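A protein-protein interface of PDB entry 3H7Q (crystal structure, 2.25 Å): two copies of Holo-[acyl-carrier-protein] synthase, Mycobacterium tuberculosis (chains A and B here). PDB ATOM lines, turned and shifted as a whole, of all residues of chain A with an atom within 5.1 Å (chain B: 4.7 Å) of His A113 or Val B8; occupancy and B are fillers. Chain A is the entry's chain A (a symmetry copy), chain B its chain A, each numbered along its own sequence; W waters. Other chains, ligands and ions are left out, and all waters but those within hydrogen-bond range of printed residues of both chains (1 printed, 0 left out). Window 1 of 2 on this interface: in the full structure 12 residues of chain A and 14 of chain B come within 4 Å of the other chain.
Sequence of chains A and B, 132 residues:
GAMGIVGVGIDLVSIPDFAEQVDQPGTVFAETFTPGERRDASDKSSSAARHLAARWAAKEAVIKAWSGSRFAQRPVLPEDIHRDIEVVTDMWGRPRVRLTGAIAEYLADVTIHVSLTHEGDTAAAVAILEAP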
ATOM      1  N   THR A 111     -15.907  15.279  24.861  1.00  0.00           N
ATOM      2  CA  THR A 111     -16.308  16.655  24.595  1.00  0.00           C
ATOM      3  C   THR A 111     -16.105  16.992  23.129  1.00  0.00           C
ATOM      4  O   THR A 111     -15.035  16.753  22.571  1.00  0.00           O
ATOM      5  CB  THR A 111     -15.536  17.651  25.464  1.00  0.00           C
ATOM      6  OG1 THR A 111     -15.703  17.309  26.849  1.00  0.00           O
ATOM      7  CG2 THR A 111     -16.042  19.068  25.218  1.00  0.00           C
ATOM      8  N   ILE A 112     -17.144  17.542  22.510  1.00  0.00           N
ATOM      9  CA  ILE A 112     -17.139  17.801  21.078  1.00  0.00           C
ATOM     10  C   ILE A 112     -17.090  19.292  20.785  1.00  0.00           C
ATOM     11  O   ILE A 112     -17.945  20.061  21.241  1.00  0.00           O
ATOM     12  CB  ILE A 112     -18.391  17.227  20.407  1.00  0.00           C
ATOM     13  CG1 ILE A 112     -18.522  15.731  20.711  1.00  0.00           C
ATOM     14  CG2 ILE A 112     -18.355  17.491  18.900  1.00  0.00           C
ATOM     15  CD1 ILE A 112     -19.875  15.157  20.356  1.00  0.00           C
ATOM     16  N   HIS A 113     -16.072  19.690  20.034  1.00  0.00           N
ATOM     17  CA  HIS A 113     -15.915  21.062  19.587  1.00  0.00           C
ATOM     18  C   HIS A 113     -16.091  21.075  18.079  1.00  0.00           C
ATOM     19  O   HIS A 113     -15.424  20.332  17.366  1.00  0.00           O
ATOM     20  CB  HIS A 113     -14.520  21.588  19.917  1.00  0.00           C
ATOM     21  CG  HIS A 113     -14.117  21.419  21.352  1.00  0.00           C
ATOM     22  ND1 HIS A 113     -14.303  22.403  22.302  1.00  0.00           N
ATOM     23  CD2 HIS A 113     -13.485  20.399  21.984  1.00  0.00           C
ATOM     24  CE1 HIS A 113     -13.824  21.988  23.461  1.00  0.00           C
ATOM     25  NE2 HIS A 113     -13.319  20.779  23.295  1.00  0.00           N
ATOM     26  N   VAL A 114     -16.996  21.912  17.595  1.00  0.00           N
ATOM     27  CA  VAL A 114     -17.223  22.031  16.161  1.00  0.00           C
ATOM     28  C   VAL A 114     -17.323  23.505  15.784  1.00  0.00           C
ATOM     29  O   VAL A 114     -17.823  24.321  16.559  1.00  0.00           O
ATOM     30  CB  VAL A 114     -18.514  21.293  15.727  1.00  0.00           C
ATOM     31  CG1 VAL A 114     -19.747  21.953  16.356  1.00  0.00           C
ATOM     32  CG2 VAL A 114     -18.645  21.290  14.224  1.00  0.00           C
ATOM     33  N   SER A 115     -16.834  23.839  14.597  1.00  0.00           N
ATOM     34  CA  SER A 115     -16.957  25.192  14.057  1.00  0.00           C
ATOM     35  C   SER A 115     -17.233  25.105  12.552  1.00  0.00           C
ATOM     36  O   SER A 115     -16.665  24.266  11.854  1.00  0.00           O
ATOM     37  CB  SER A 115     -15.688  26.003  14.338  1.00  0.00           C
ATOM     38  OG  SER A 115     -15.740  27.278  13.721  1.00  0.00           O
ATOM     39  N   VAL A 126     -14.797  22.187  10.905  1.00  0.00           N
ATOM     40  CA  VAL A 126     -13.790  21.397  11.600  1.00  0.00           C
ATOM     41  C   VAL A 126     -14.345  20.897  12.927  1.00  0.00           C
ATOM     42  O   VAL A 126     -15.089  21.601  13.604  1.00  0.00           O
ATOM     43  CB  VAL A 126     -12.496  22.198  11.849  1.00  0.00           C
ATOM     44  CG1 VAL A 126     -12.776  23.450  12.682  1.00  0.00           C
ATOM     45  CG2 VAL A 126     -11.452  21.319  12.523  1.00  0.00           C
ATOM     46  N   ALA A 127     -13.992  19.670  13.287  1.00  0.00           N
ATOM     47  CA  ALA A 127     -14.435  19.095  14.551  1.00  0.00           C
ATOM     48  C   ALA A 127     -13.255  18.494  15.300  1.00  0.00           C
ATOM     49  O   ALA A 127     -12.375  17.875  14.698  1.00  0.00           O
ATOM     50  CB  ALA A 127     -15.510  18.051  14.316  1.00  0.00           C
ATOM     51  N   ILE A 128     -13.237  18.693  16.615  1.00  0.00           N
ATOM     52  CA  ILE A 128     -12.211  18.109  17.477  1.00  0.00           C
ATOM     53  C   ILE A 128     -12.831  17.396  18.674  1.00  0.00           C
ATOM     54  O   ILE A 128     -13.582  18.002  19.440  1.00  0.00           O
ATOM     55  CB  ILE A 128     -11.248  19.183  17.990  1.00  0.00           C
ATOM     56  CG1 ILE A 128     -10.839  20.111  16.842  1.00  0.00           C
ATOM     57  CG2 ILE A 128     -10.029  18.542  18.654  1.00  0.00           C
ATOM     58  CD1 ILE A 128      -9.799  21.119  17.222  1.00  0.00           C
ATOM     59  N   GLU A 130     -12.393  15.389  22.315  1.00  0.00           N
ATOM     60  CA  GLU A 130     -11.521  15.588  23.475  1.00  0.00           C
ATOM     61  C   GLU A 130     -12.007  14.736  24.660  1.00  0.00           C
ATOM     62  O   GLU A 130     -13.209  14.568  24.855  1.00  0.00           O
ATOM     63  CB  GLU A 130     -11.538  17.074  23.867  1.00  0.00           C
ATOM     64  CG  GLU A 130     -10.265  17.600  24.500  1.00  0.00           C
ATOM     65  CD  GLU A 130     -10.377  19.056  24.966  1.00  0.00           C
ATOM     66  OE1 GLU A 130     -11.491  19.521  25.272  1.00  0.00           O
ATOM     67  OE2 GLU A 130      -9.341  19.738  25.046  1.00  0.00           O
ATOM     68  N   ILE B   5      -9.279  22.327  25.865  1.00  0.00           N
ATOM     69  CA  ILE B   5      -9.671  23.220  24.786  1.00  0.00           C
ATOM     70  C   ILE B   5     -10.846  24.084  25.222  1.00  0.00           C
ATOM     71  O   ILE B   5     -11.825  23.583  25.767  1.00  0.00           O
ATOM     72  CB  ILE B   5     -10.033  22.440  23.505  1.00  0.00           C
ATOM     73  CG1 ILE B   5      -8.777  21.817  22.897  1.00  0.00           C
ATOM     74  CG2 ILE B   5     -10.735  23.353  22.489  1.00  0.00           C
ATOM     75  CD1 ILE B   5      -9.063  20.942  21.695  1.00  0.00           C
ATOM     76  N   GLY B   7     -12.178  26.764  23.018  1.00  0.00           N
ATOM     77  CA  GLY B   7     -12.941  27.234  21.875  1.00  0.00           C
ATOM     78  C   GLY B   7     -12.269  26.883  20.559  1.00  0.00           C
ATOM     79  O   GLY B   7     -11.052  26.697  20.513  1.00  0.00           O
ATOM     80  N   VAL B   8     -13.062  26.786  19.493  1.00  0.00           N
ATOM     81  CA  VAL B   8     -12.543  26.499  18.157  1.00  0.00           C
ATOM     82  C   VAL B   8     -13.226  27.373  17.100  1.00  0.00           C
ATOM     83  O   VAL B   8     -14.389  27.749  17.248  1.00  0.00           O
ATOM     84  CB  VAL B   8     -12.706  25.011  17.780  1.00  0.00           C
ATOM     85  CG1 VAL B   8     -11.889  24.676  16.529  1.00  0.00           C
ATOM     86  CG2 VAL B   8     -12.278  24.131  18.931  1.00  0.00           C
ATOM     87  N   GLY B   9     -12.496  27.699  16.039  1.00  0.00           N
ATOM     88  CA  GLY B   9     -13.013  28.592  15.018  1.00  0.00           C
ATOM     89  C   GLY B   9     -12.400  28.329  13.660  1.00  0.00           C
ATOM     90  O   GLY B   9     -11.198  28.123  13.554  1.00  0.00           O
ATOM     91  N   ILE B  10     -13.228  28.308  12.621  1.00  0.00           N
ATOM     92  CA  ILE B  10     -12.704  28.210  11.263  1.00  0.00           C
ATOM     93  C   ILE B  10     -13.341  29.289  10.390  1.00  0.00           C
ATOM     94  O   ILE B  10     -14.505  29.621  10.573  1.00  0.00           O
ATOM     95  CB  ILE B  10     -12.931  26.820  10.644  1.00  0.00           C
ATOM     96  CG1 ILE B  10     -12.167  26.704   9.320  1.00  0.00           C
ATOM     97  CG2 ILE B  10     -14.428  26.552  10.431  1.00  0.00           C
ATOM     98  CD1 ILE B  10     -12.230  25.330   8.672  1.00  0.00           C
ATOM     99  N   LYS B  64     -14.603  33.648  16.410  1.00  0.00           N
ATOM    100  CA  LYS B  64     -15.500  32.501  16.541  1.00  0.00           C
ATOM    101  C   LYS B  64     -15.134  31.626  17.732  1.00  0.00           C
ATOM    102  O   LYS B  64     -16.006  31.169  18.471  1.00  0.00           O
ATOM    103  CB  LYS B  64     -15.515  31.655  15.265  1.00  0.00           C
ATOM    104  CG  LYS B  64     -16.486  32.152  14.212  1.00  0.00           C
ATOM    105  CD  LYS B  64     -16.314  31.401  12.896  1.00  0.00           C
ATOM    106  CE  LYS B  64     -16.945  32.165  11.737  1.00  0.00           C
ATOM    107  NZ  LYS B  64     -16.655  31.524  10.421  1.00  0.00           N
ATOM    108  N   ALA B  65     -13.842  31.382  17.910  1.00  0.00           N
ATOM    109  CA  ALA B  65     -13.395  30.529  19.003  1.00  0.00           C
ATOM    110  C   ALA B  65     -13.763  31.144  20.356  1.00  0.00           C
ATOM    111  O   ALA B  65     -14.132  30.441  21.288  1.00  0.00           O
ATOM    112  CB  ALA B  65     -11.901  30.293  18.908  1.00  0.00           C
ATOM    113  N   ALA B 127      -8.533  28.678  14.378  1.00  0.00           N
ATOM    114  CA  ALA B 127      -8.039  29.112  15.678  1.00  0.00           C
ATOM    115  C   ALA B 127      -8.523  28.168  16.769  1.00  0.00           C
ATOM    116  O   ALA B 127      -9.667  27.710  16.745  1.00  0.00           O
ATOM    117  CB  ALA B 127      -8.476  30.536  15.969  1.00  0.00           C
ATOM    118  N   ILE B 128      -7.639  27.870  17.716  1.00  0.00           N
ATOM    119  CA  ILE B 128      -7.982  27.041  18.870  1.00  0.00           C
ATOM    120  C   ILE B 128      -7.552  27.701  20.176  1.00  0.00           C
ATOM    121  O   ILE B 128      -6.378  28.022  20.355  1.00  0.00           O
ATOM    122  CB  ILE B 128      -7.319  25.664  18.775  1.00  0.00           C
ATOM    123  CG1 ILE B 128      -7.481  25.102  17.359  1.00  0.00           C
ATOM    124  CG2 ILE B 128      -7.895  24.714  19.824  1.00  0.00           C
ATOM    125  CD1 ILE B 128      -6.972  23.703  17.203  1.00  0.00           C
HETATM  126  O   HOH W   1     -12.154  21.295  27.341  1.00  0.00           O
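A ring nitrogen (NE2) of His A113 lies within hydrogen-bond range of the side-chain carboxylate of Glu A130.
The backbone carbonyl oxygen (O) of His A113 lies within hydrogen-bond range of the backbone NH (N) of Ile A128 (2.8 Å).
O of Ile B10 sits at hydrogen-bond distance from NZ of Lys B64 (2.9 Å).
The backbone carbonyl oxygen (O) of Gly B9 is in hydrogen-bond range of the backbone NH (N) of Ala B127.
The backbone NH of Thr A111 lies within hydrogen-bond range of the backbone carbonyl oxygen of Glu A130 (2.8 Å).
O of Ser A115 is in hydrogen-bond range of N of Val A126 (3.0 Å).
Ile A128 touches its own counterpart, Ile B128.
Positions printed for both chains: 127 and 128.
Of the 9 pairs that touch across the chains among the printed residues, 1 has its exchanged pair printed and touching as well.
Among the printed residues, merely in contact across the chains: Ser A115 with Gly B9, His A113 with Ile B5, His A113 with Val B8, Ser A115 with Val B8, Ile A128 with Ile B128, Val A126 with Ile B10 and Ile A128 with Ile B5.
OE2 of Glu A130 sits at hydrogen-bond distance from N of Ile B5 (2.7 Å).
OG of Ser A115 lies within hydrogen-bond range of N of Ile B10 (2.9 Å).
Of chain B, only Ile B5 (3.4 Å) and Val B8 (3.5 Å) come within 4 Å of His A113.
Ala A127 touches none of the printed residues of chain B.
Printed residues of chain B within 4 Å of Ile A128: Ile B5 (3.99 Å) and Ile B128 (3.8 Å).
Of the printed residues of chain B, Glu A130 touches Ile B5.
Of the printed residues of chain A, Ile B5 touches His A113 (3.4 Å), Ile A128 (3.99 Å) and Glu A130 (2.7 Å).
Of chain A, only His A113 and Ser A115 come within 4 Å of Val B8.
Of the printed residues of chain A, Ile B10 touches Ser A115 and Val A126.
Ala B65 touches none of the printed residues of chain A.
Of the printed residues of chain A, Ile B128 touches Ile A128.
The nearest printed residue of chain B that does not touch His A113 is Gly B7 (4.9 Å).
Of the 9 printed residues of chain B, 5 touch a printed residue of chain A.
Of the 9 printed residues of chain A, 5 touch a printed residue of chain B.
Hydrophobic or aromatic side chains of chain A that line the printed part of chain B: His A113, Val A126 and Ile A128.
Water W1 bridges O of Ile B5 (2.8 Å) and OE1 of Glu A130 (2.8 Å).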
